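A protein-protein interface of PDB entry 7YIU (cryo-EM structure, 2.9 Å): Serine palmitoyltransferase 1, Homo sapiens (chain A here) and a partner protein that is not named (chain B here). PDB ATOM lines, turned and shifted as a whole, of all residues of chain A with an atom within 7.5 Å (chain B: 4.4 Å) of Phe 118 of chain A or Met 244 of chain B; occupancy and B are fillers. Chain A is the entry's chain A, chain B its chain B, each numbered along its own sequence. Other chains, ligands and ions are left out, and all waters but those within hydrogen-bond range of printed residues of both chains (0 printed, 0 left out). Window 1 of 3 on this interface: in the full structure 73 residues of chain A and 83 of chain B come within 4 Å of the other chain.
NE2 of His 403 of chain B is in hydrogen-bond range of OE2 of Glu 385 of chain A (3.0 Å).
The side-chain hydroxyl of Ser 404 of chain B lies within hydrogen-bond range of the side-chain hydroxyl of Tyr 116 of chain A (3.1 Å).
The side-chain hydroxyl (OH) of Tyr 407 of chain B is in hydrogen-bond range of the backbone NH (N) of Leu 382 of chain A.
OG of Ser 402 of chain B sits close to N of Ser 404 of chain B (3.3 Å).
Ala 240 of chain B touches Tyr 116 of chain A (CB to CE2, 3.9 Å).
OH of Tyr 116 of chain A touches CB of Ala 408 of chain B, at 3.2 Å.
Phe 118 of chain A touches Met 244 of chain B.
CE1 of Phe 118 of chain A touches CB of Tyr 407 of chain B (3.8 Å).
ND1 of His 403 of chain B touches CE2 of Phe 143 of chain A, 3.9 Å away.
CD2 of Tyr 407 of chain B touches CD2 of Phe 143 of chain A, 3.6 Å away.
CD1 of Leu 382 of chain A touches CD2 of His 403 of chain B, at 3.5 Å.
Glu 385 of chain A touches Pro 247 of chain B.
Phe 118 of chain A touches two residues of chain B.
Of the printed residues of chain B, Phe 143 of chain A touches His 403 (3.9 Å) and Tyr 407 (3.6 Å).
Lys 147 of chain A touches none of the printed residues of chain B.
Gly 265 of chain A touches none of the printed residues of chain B.
Of chain A, only Phe 118 (3.7 Å) comes within 4 Å of Met 244 of chain B.
Printed residues of chain A within 4 Å of Ser 404 of chain B: Tyr 116 (3.1 Å).
Of the 23 printed residues of chain A, 5 touch a printed residue of chain B.
Hydrophobic or aromatic side chains of chain A within 4 Å of the printed part of chain B: Tyr 116, Phe 118, Phe 143 and Leu 382.
Of the 12 printed residues of chain B, 7 touch a printed residue of chain A.
Hydrophobic or aromatic side chains of chain B within 4 Å of the printed part of chain A: Ala 240, Met 244, His 403, Tyr 407 and Ala 408.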
ATOM      1  N   TYR A 114       4.374 -38.418   8.460  1.00  0.00           N
ATOM      2  CA  TYR A 114       4.478 -37.016   8.096  1.00  0.00           C
ATOM      3  C   TYR A 114       4.917 -36.910   6.642  1.00  0.00           C
ATOM      4  O   TYR A 114       5.277 -37.899   6.007  1.00  0.00           O
ATOM      5  CB  TYR A 114       5.479 -36.289   8.999  1.00  0.00           C
ATOM      6  CG  TYR A 114       5.033 -36.081  10.428  1.00  0.00           C
ATOM      7  CD1 TYR A 114       4.740 -34.816  10.901  1.00  0.00           C
ATOM      8  CD2 TYR A 114       4.930 -37.143  11.309  1.00  0.00           C
ATOM      9  CE1 TYR A 114       4.347 -34.617  12.199  1.00  0.00           C
ATOM     10  CE2 TYR A 114       4.532 -36.953  12.606  1.00  0.00           C
ATOM     11  CZ  TYR A 114       4.243 -35.688  13.047  1.00  0.00           C
ATOM     12  OH  TYR A 114       3.846 -35.487  14.342  1.00  0.00           O
ATOM     13  N   SER A 115       4.894 -35.693   6.113  1.00  0.00           N
ATOM     14  CA  SER A 115       5.275 -35.481   4.723  1.00  0.00           C
ATOM     15  C   SER A 115       6.661 -34.873   4.554  1.00  0.00           C
ATOM     16  O   SER A 115       7.035 -34.533   3.429  1.00  0.00           O
ATOM     17  CB  SER A 115       4.248 -34.591   4.026  1.00  0.00           C
ATOM     18  OG  SER A 115       4.236 -33.297   4.588  1.00  0.00           O
ATOM     19  N   TYR A 116       7.424 -34.726   5.629  1.00  0.00           N
ATOM     20  CA  TYR A 116       8.753 -34.143   5.582  1.00  0.00           C
ATOM     21  C   TYR A 116       9.605 -34.770   6.670  1.00  0.00           C
ATOM     22  O   TYR A 116       9.180 -34.858   7.823  1.00  0.00           O
ATOM     23  CB  TYR A 116       8.667 -32.643   5.777  1.00  0.00           C
ATOM     24  CG  TYR A 116       9.793 -31.820   5.211  1.00  0.00           C
ATOM     25  CD1 TYR A 116      10.088 -31.856   3.863  1.00  0.00           C
ATOM     26  CD2 TYR A 116      10.512 -30.951   6.011  1.00  0.00           C
ATOM     27  CE1 TYR A 116      11.094 -31.091   3.337  1.00  0.00           C
ATOM     28  CE2 TYR A 116      11.516 -30.176   5.492  1.00  0.00           C
ATOM     29  CZ  TYR A 116      11.803 -30.249   4.152  1.00  0.00           C
ATOM     30  OH  TYR A 116      12.806 -29.482   3.615  1.00  0.00           O
ATOM     31  N   GLY A 117      10.802 -35.207   6.305  1.00  0.00           N
ATOM     32  CA  GLY A 117      11.636 -35.912   7.254  1.00  0.00           C
ATOM     33  C   GLY A 117      12.168 -35.082   8.396  1.00  0.00           C
ATOM     34  O   GLY A 117      12.419 -35.631   9.471  1.00  0.00           O
ATOM     35  N   PHE A 118      12.352 -33.781   8.199  1.00  0.00           N
ATOM     36  CA  PHE A 118      12.829 -32.914   9.263  1.00  0.00           C
ATOM     37  C   PHE A 118      11.782 -32.667  10.337  1.00  0.00           C
ATOM     38  O   PHE A 118      12.127 -32.608  11.519  1.00  0.00           O
ATOM     39  CB  PHE A 118      13.273 -31.565   8.687  1.00  0.00           C
ATOM     40  CG  PHE A 118      14.044 -30.703   9.654  1.00  0.00           C
ATOM     41  CD1 PHE A 118      15.421 -30.666   9.613  1.00  0.00           C
ATOM     42  CD2 PHE A 118      13.392 -29.932  10.603  1.00  0.00           C
ATOM     43  CE1 PHE A 118      16.130 -29.875  10.483  1.00  0.00           C
ATOM     44  CE2 PHE A 118      14.097 -29.138  11.474  1.00  0.00           C
ATOM     45  CZ  PHE A 118      15.468 -29.113  11.417  1.00  0.00           C
ATOM     46  N   ALA A 119      10.516 -32.533   9.955  1.00  0.00           N
ATOM     47  CA  ALA A 119       9.466 -32.102  10.864  1.00  0.00           C
ATOM     48  C   ALA A 119       8.830 -33.242  11.641  1.00  0.00           C
ATOM     49  O   ALA A 119       7.960 -32.986  12.473  1.00  0.00           O
ATOM     50  CB  ALA A 119       8.388 -31.348  10.090  1.00  0.00           C
ATOM     51  N   THR A 120       9.228 -34.487  11.399  1.00  0.00           N
ATOM     52  CA  THR A 120       8.593 -35.591  12.107  1.00  0.00           C
ATOM     53  C   THR A 120       9.001 -35.620  13.574  1.00  0.00           C
ATOM     54  O   THR A 120       8.193 -35.968  14.437  1.00  0.00           O
ATOM     55  CB  THR A 120       8.912 -36.922  11.424  1.00  0.00           C
ATOM     56  OG1 THR A 120       8.330 -37.993  12.171  1.00  0.00           O
ATOM     57  CG2 THR A 120      10.396 -37.149  11.336  1.00  0.00           C
ATOM     58  N   ILE A 121      10.248 -35.253  13.878  1.00  0.00           N
ATOM     59  CA  ILE A 121      10.712 -35.215  15.265  1.00  0.00           C
ATOM     60  C   ILE A 121      10.736 -33.800  15.823  1.00  0.00           C
ATOM     61  O   ILE A 121      10.726 -33.627  17.050  1.00  0.00           O
ATOM     62  CB  ILE A 121      12.096 -35.883  15.378  1.00  0.00           C
ATOM     63  CG1 ILE A 121      12.484 -36.120  16.840  1.00  0.00           C
ATOM     64  CG2 ILE A 121      13.148 -35.072  14.667  1.00  0.00           C
ATOM     65  CD1 ILE A 121      11.649 -37.163  17.537  1.00  0.00           C
ATOM     66  N   ALA A 122      10.749 -32.782  14.972  1.00  0.00           N
ATOM     67  CA  ALA A 122      10.584 -31.411  15.424  1.00  0.00           C
ATOM     68  C   ALA A 122       9.145 -31.090  15.786  1.00  0.00           C
ATOM     69  O   ALA A 122       8.893 -30.040  16.383  1.00  0.00           O
ATOM     70  CB  ALA A 122      11.070 -30.438  14.352  1.00  0.00           C
ATOM     71  N   SER A 123       8.200 -31.962  15.435  1.00  0.00           N
ATOM     72  CA  SER A 123       6.805 -31.818  15.817  1.00  0.00           C
ATOM     73  C   SER A 123       6.360 -32.828  16.861  1.00  0.00           C
ATOM     74  O   SER A 123       5.322 -32.619  17.490  1.00  0.00           O
ATOM     75  CB  SER A 123       5.895 -31.957  14.592  1.00  0.00           C
ATOM     76  OG  SER A 123       5.985 -30.824  13.754  1.00  0.00           O
ATOM     77  N   CYS A 142      21.237 -34.458  16.825  1.00  0.00           N
ATOM     78  CA  CYS A 142      21.224 -33.742  15.560  1.00  0.00           C
ATOM     79  C   CYS A 142      20.414 -32.454  15.669  1.00  0.00           C
ATOM     80  O   CYS A 142      19.883 -32.107  16.723  1.00  0.00           O
ATOM     81  CB  CYS A 142      20.669 -34.631  14.453  1.00  0.00           C
ATOM     82  SG  CYS A 142      19.017 -35.273  14.757  1.00  0.00           S
ATOM     83  N   PHE A 143      20.322 -31.737  14.545  1.00  0.00           N
ATOM     84  CA  PHE A 143      19.704 -30.416  14.553  1.00  0.00           C
ATOM     85  C   PHE A 143      18.194 -30.487  14.718  1.00  0.00           C
ATOM     86  O   PHE A 143      17.599 -29.611  15.355  1.00  0.00           O
ATOM     87  CB  PHE A 143      20.051 -29.673  13.271  1.00  0.00           C
ATOM     88  CG  PHE A 143      19.818 -28.198  13.344  1.00  0.00           C
ATOM     89  CD1 PHE A 143      20.637 -27.392  14.102  1.00  0.00           C
ATOM     90  CD2 PHE A 143      18.784 -27.614  12.640  1.00  0.00           C
ATOM     91  CE1 PHE A 143      20.426 -26.042  14.161  1.00  0.00           C
ATOM     92  CE2 PHE A 143      18.572 -26.266  12.697  1.00  0.00           C
ATOM     93  CZ  PHE A 143      19.395 -25.478  13.455  1.00  0.00           C
ATOM     94  N   ALA A 144      17.554 -31.507  14.147  1.00  0.00           N
ATOM     95  CA  ALA A 144      16.106 -31.634  14.269  1.00  0.00           C
ATOM     96  C   ALA A 144      15.691 -31.825  15.721  1.00  0.00           C
ATOM     97  O   ALA A 144      14.698 -31.243  16.172  1.00  0.00           O
ATOM     98  CB  ALA A 144      15.610 -32.790  13.409  1.00  0.00           C
ATOM     99  N   ILE A 145      16.447 -32.626  16.470  1.00  0.00           N
ATOM    100  CA  ILE A 145      16.170 -32.802  17.889  1.00  0.00           C
ATOM    101  C   ILE A 145      16.324 -31.481  18.631  1.00  0.00           C
ATOM    102  O   ILE A 145      15.512 -31.148  19.498  1.00  0.00           O
ATOM    103  CB  ILE A 145      17.082 -33.893  18.476  1.00  0.00           C
ATOM    104  CG1 ILE A 145      16.528 -35.276  18.157  1.00  0.00           C
ATOM    105  CG2 ILE A 145      17.212 -33.735  19.970  1.00  0.00           C
ATOM    106  CD1 ILE A 145      17.555 -36.362  18.225  1.00  0.00           C
ATOM    107  N   GLN A 146      17.365 -30.711  18.313  1.00  0.00           N
ATOM    108  CA  GLN A 146      17.564 -29.435  18.990  1.00  0.00           C
ATOM    109  C   GLN A 146      16.416 -28.475  18.717  1.00  0.00           C
ATOM    110  O   GLN A 146      15.956 -27.779  19.627  1.00  0.00           O
ATOM    111  CB  GLN A 146      18.883 -28.804  18.559  1.00  0.00           C
ATOM    112  CG  GLN A 146      20.104 -29.660  18.757  1.00  0.00           C
ATOM    113  CD  GLN A 146      21.337 -29.006  18.178  1.00  0.00           C
ATOM    114  OE1 GLN A 146      21.422 -27.783  18.111  1.00  0.00           O
ATOM    115  NE2 GLN A 146      22.290 -29.814  17.736  1.00  0.00           N
ATOM    116  N   LYS A 147      15.950 -28.407  17.468  1.00  0.00           N
ATOM    117  CA  LYS A 147      14.818 -27.534  17.166  1.00  0.00           C
ATOM    118  C   LYS A 147      13.544 -28.001  17.854  1.00  0.00           C
ATOM    119  O   LYS A 147      12.777 -27.173  18.358  1.00  0.00           O
ATOM    120  CB  LYS A 147      14.594 -27.433  15.660  1.00  0.00           C
ATOM    121  CG  LYS A 147      15.730 -26.795  14.896  1.00  0.00           C
ATOM    122  CD  LYS A 147      15.926 -25.337  15.270  1.00  0.00           C
ATOM    123  CE  LYS A 147      17.175 -25.154  16.120  1.00  0.00           C
ATOM    124  NZ  LYS A 147      17.540 -23.737  16.327  1.00  0.00           N
ATOM    125  N   GLY A 148      13.296 -29.311  17.883  1.00  0.00           N
ATOM    126  CA  GLY A 148      12.162 -29.827  18.622  1.00  0.00           C
ATOM    127  C   GLY A 148      12.210 -29.550  20.106  1.00  0.00           C
ATOM    128  O   GLY A 148      11.167 -29.300  20.711  1.00  0.00           O
ATOM    129  N   ASN A 256      12.819 -41.529   9.471  1.00  0.00           N
ATOM    130  CA  ASN A 256      12.384 -40.915   8.226  1.00  0.00           C
ATOM    131  C   ASN A 256      12.439 -41.929   7.093  1.00  0.00           C
ATOM    132  O   ASN A 256      13.101 -42.965   7.184  1.00  0.00           O
ATOM    133  CB  ASN A 256      13.198 -39.651   7.885  1.00  0.00           C
ATOM    134  CG  ASN A 256      14.643 -39.934   7.546  1.00  0.00           C
ATOM    135  OD1 ASN A 256      15.070 -41.079   7.454  1.00  0.00           O
ATOM    136  ND2 ASN A 256      15.410 -38.872   7.358  1.00  0.00           N
ATOM    137  N   GLU A 258      13.580 -41.446   4.020  1.00  0.00           N
ATOM    138  CA  GLU A 258      14.396 -40.767   3.023  1.00  0.00           C
ATOM    139  C   GLU A 258      15.790 -41.358   2.872  1.00  0.00           C
ATOM    140  O   GLU A 258      16.532 -40.929   1.987  1.00  0.00           O
ATOM    141  CB  GLU A 258      14.511 -39.282   3.369  1.00  0.00           C
ATOM    142  CG  GLU A 258      13.193 -38.552   3.381  1.00  0.00           C
ATOM    143  CD  GLU A 258      13.307 -37.147   3.919  1.00  0.00           C
ATOM    144  OE1 GLU A 258      14.365 -36.815   4.487  1.00  0.00           O
ATOM    145  OE2 GLU A 258      12.340 -36.373   3.772  1.00  0.00           O
ATOM    146  N   GLY A 265       9.663 -38.206   3.347  1.00  0.00           N
ATOM    147  CA  GLY A 265       8.798 -38.166   4.510  1.00  0.00           C
ATOM    148  C   GLY A 265       9.421 -38.854   5.711  1.00  0.00           C
ATOM    149  O   GLY A 265      10.524 -39.395   5.659  1.00  0.00           O
ATOM    150  N   GLY A 266       8.674 -38.825   6.809  1.00  0.00           N
ATOM    151  CA  GLY A 266       9.089 -39.505   8.020  1.00  0.00           C
ATOM    152  C   GLY A 266       7.912 -40.202   8.662  1.00  0.00           C
ATOM    153  O   GLY A 266       6.764 -40.012   8.259  1.00  0.00           O
ATOM    154  N   LEU A 382      25.607 -25.508  10.637  1.00  0.00           N
ATOM    155  CA  LEU A 382      25.334 -24.088  10.830  1.00  0.00           C
ATOM    156  C   LEU A 382      26.103 -23.655  12.075  1.00  0.00           C
ATOM    157  O   LEU A 382      25.664 -23.862  13.203  1.00  0.00           O
ATOM    158  CB  LEU A 382      23.843 -23.839  10.970  1.00  0.00           C
ATOM    159  CG  LEU A 382      23.066 -23.495   9.700  1.00  0.00           C
ATOM    160  CD1 LEU A 382      21.681 -23.024  10.055  1.00  0.00           C
ATOM    161  CD2 LEU A 382      23.793 -22.445   8.899  1.00  0.00           C
ATOM    162  N   GLU A 385      24.415 -21.216  14.808  1.00  0.00           N
ATOM    163  CA  GLU A 385      23.162 -21.706  15.376  1.00  0.00           C
ATOM    164  C   GLU A 385      23.280 -23.203  15.647  1.00  0.00           C
ATOM    165  O   GLU A 385      22.628 -24.005  14.982  1.00  0.00           O
ATOM    166  CB  GLU A 385      21.993 -21.401  14.434  1.00  0.00           C
ATOM    167  CG  GLU A 385      21.799 -19.924  14.150  1.00  0.00           C
ATOM    168  CD  GLU A 385      20.488 -19.623  13.448  1.00  0.00           C
ATOM    169  OE1 GLU A 385      20.394 -18.570  12.782  1.00  0.00           O
ATOM    170  OE2 GLU A 385      19.549 -20.436  13.560  1.00  0.00           O
ATOM    171  N   ALA B 240       7.353 -25.739   6.064  1.00  0.00           N
ATOM    172  CA  ALA B 240       8.752 -25.562   6.431  1.00  0.00           C
ATOM    173  C   ALA B 240       9.423 -24.378   5.751  1.00  0.00           C
ATOM    174  O   ALA B 240      10.552 -24.042   6.067  1.00  0.00           O
ATOM    175  CB  ALA B 240       9.529 -26.836   6.153  1.00  0.00           C
ATOM    176  N   ASN B 242       8.250 -21.354   5.903  1.00  0.00           N
ATOM    177  CA  ASN B 242       8.059 -20.266   6.843  1.00  0.00           C
ATOM    178  C   ASN B 242       8.735 -20.500   8.184  1.00  0.00           C
ATOM    179  O   ASN B 242       9.360 -19.605   8.735  1.00  0.00           O
ATOM    180  CB  ASN B 242       6.569 -20.056   7.079  1.00  0.00           C
ATOM    181  CG  ASN B 242       5.950 -19.117   6.076  1.00  0.00           C
ATOM    182  OD1 ASN B 242       4.738 -19.102   5.893  1.00  0.00           O
ATOM    183  ND2 ASN B 242       6.780 -18.324   5.423  1.00  0.00           N
ATOM    184  N   SER B 243       8.614 -21.709   8.705  1.00  0.00           N
ATOM    185  CA  SER B 243       9.179 -22.036  10.007  1.00  0.00           C
ATOM    186  C   SER B 243      10.683 -22.270  10.034  1.00  0.00           C
ATOM    187  O   SER B 243      11.269 -22.352  11.105  1.00  0.00           O
ATOM    188  CB  SER B 243       8.445 -23.231  10.613  1.00  0.00           C
ATOM    189  OG  SER B 243       9.220 -24.408  10.526  1.00  0.00           O
ATOM    190  N   MET B 244      11.312 -22.370   8.871  1.00  0.00           N
ATOM    191  CA  MET B 244      12.751 -22.602   8.819  1.00  0.00           C
ATOM    192  C   MET B 244      13.519 -21.473   8.151  1.00  0.00           C
ATOM    193  O   MET B 244      14.730 -21.551   8.007  1.00  0.00           O
ATOM    194  CB  MET B 244      13.048 -23.911   8.093  1.00  0.00           C
ATOM    195  CG  MET B 244      13.206 -25.109   9.006  1.00  0.00           C
ATOM    196  SD  MET B 244      12.842 -26.649   8.156  1.00  0.00           S
ATOM    197  CE  MET B 244      14.469 -27.376   8.036  1.00  0.00           C
ATOM    198  N   ASN B 245      12.817 -20.423   7.747  1.00  0.00           N
ATOM    199  CA  ASN B 245      13.459 -19.295   7.083  1.00  0.00           C
ATOM    200  C   ASN B 245      13.215 -17.965   7.780  1.00  0.00           C
ATOM    201  O   ASN B 245      13.929 -17.008   7.538  1.00  0.00           O
ATOM    202  CB  ASN B 245      13.002 -19.201   5.630  1.00  0.00           C
ATOM    203  CG  ASN B 245      13.582 -20.294   4.765  1.00  0.00           C
ATOM    204  OD1 ASN B 245      14.754 -20.631   4.875  1.00  0.00           O
ATOM    205  ND2 ASN B 245      12.759 -20.856   3.899  1.00  0.00           N
ATOM    206  N   ILE B 246      12.203 -17.903   8.640  1.00  0.00           N
ATOM    207  CA  ILE B 246      11.909 -16.667   9.352  1.00  0.00           C
ATOM    208  C   ILE B 246      12.935 -16.422  10.446  1.00  0.00           C
ATOM    209  O   ILE B 246      13.272 -15.283  10.729  1.00  0.00           O
ATOM    210  CB  ILE B 246      10.486 -16.635   9.935  1.00  0.00           C
ATOM    211  CG1 ILE B 246       9.468 -16.389   8.825  1.00  0.00           C
ATOM    212  CG2 ILE B 246      10.370 -15.536  10.975  1.00  0.00           C
ATOM    213  CD1 ILE B 246       8.041 -16.279   9.309  1.00  0.00           C
ATOM    214  N   PRO B 247      13.452 -17.501  11.062  1.00  0.00           N
ATOM    215  CA  PRO B 247      14.484 -17.394  12.105  1.00  0.00           C
ATOM    216  C   PRO B 247      15.897 -17.125  11.576  1.00  0.00           C
ATOM    217  O   PRO B 247      16.800 -16.933  12.377  1.00  0.00           O
ATOM    218  CB  PRO B 247      14.435 -18.758  12.796  1.00  0.00           C
ATOM    219  CG  PRO B 247      13.799 -19.670  11.819  1.00  0.00           C
ATOM    220  CD  PRO B 247      12.833 -18.835  11.042  1.00  0.00           C
ATOM    221  N   SER B 402      20.141 -20.955   5.605  1.00  0.00           N
ATOM    222  CA  SER B 402      18.794 -21.419   5.907  1.00  0.00           C
ATOM    223  C   SER B 402      18.860 -22.847   6.434  1.00  0.00           C
ATOM    224  O   SER B 402      19.657 -23.644   5.965  1.00  0.00           O
ATOM    225  CB  SER B 402      17.905 -21.328   4.670  1.00  0.00           C
ATOM    226  OG  SER B 402      17.070 -22.458   4.535  1.00  0.00           O
ATOM    227  N   HIS B 403      18.016 -23.169   7.407  1.00  0.00           N
ATOM    228  CA  HIS B 403      18.006 -24.498   8.005  1.00  0.00           C
ATOM    229  C   HIS B 403      17.663 -25.622   7.032  1.00  0.00           C
ATOM    230  O   HIS B 403      18.158 -26.733   7.163  1.00  0.00           O
ATOM    231  CB  HIS B 403      17.039 -24.547   9.186  1.00  0.00           C
ATOM    232  CG  HIS B 403      17.269 -23.477  10.204  1.00  0.00           C
ATOM    233  ND1 HIS B 403      16.469 -23.326  11.315  1.00  0.00           N
ATOM    234  CD2 HIS B 403      18.203 -22.501  10.278  1.00  0.00           C
ATOM    235  CE1 HIS B 403      16.902 -22.305  12.030  1.00  0.00           C
ATOM    236  NE2 HIS B 403      17.954 -21.788  11.424  1.00  0.00           N
ATOM    237  N   SER B 404      16.808 -25.337   6.062  1.00  0.00           N
ATOM    238  CA  SER B 404      16.389 -26.345   5.103  1.00  0.00           C
ATOM    239  C   SER B 404      17.450 -26.667   4.057  1.00  0.00           C
ATOM    240  O   SER B 404      17.488 -27.768   3.521  1.00  0.00           O
ATOM    241  CB  SER B 404      15.105 -25.901   4.414  1.00  0.00           C
ATOM    242  OG  SER B 404      14.533 -26.964   3.684  1.00  0.00           O
ATOM    243  N   TYR B 407      20.123 -29.133   6.220  1.00  0.00           N
ATOM    244  CA  TYR B 407      19.720 -30.258   7.053  1.00  0.00           C
ATOM    245  C   TYR B 407      18.565 -31.083   6.511  1.00  0.00           C
ATOM    246  O   TYR B 407      18.373 -32.205   6.974  1.00  0.00           O
ATOM    247  CB  TYR B 407      19.353 -29.774   8.463  1.00  0.00           C
ATOM    248  CG  TYR B 407      20.541 -29.308   9.260  1.00  0.00           C
ATOM    249  CD1 TYR B 407      21.544 -30.188   9.621  1.00  0.00           C
ATOM    250  CD2 TYR B 407      20.662 -27.988   9.648  1.00  0.00           C
ATOM    251  CE1 TYR B 407      22.627 -29.766  10.339  1.00  0.00           C
ATOM    252  CE2 TYR B 407      21.748 -27.558  10.361  1.00  0.00           C
ATOM    253  CZ  TYR B 407      22.726 -28.450  10.705  1.00  0.00           C
ATOM    254  OH  TYR B 407      23.803 -28.019  11.432  1.00  0.00           O
ATOM    255  N   ALA B 408      17.798 -30.580   5.554  1.00  0.00           N
ATOM    256  CA  ALA B 408      16.650 -31.308   5.039  1.00  0.00           C
ATOM    257  C   ALA B 408      16.852 -31.681   3.575  1.00  0.00           C
ATOM    258  O   ALA B 408      17.547 -30.993   2.826  1.00  0.00           O
ATOM    259  CB  ALA B 408      15.378 -30.483   5.194  1.00  0.00           C
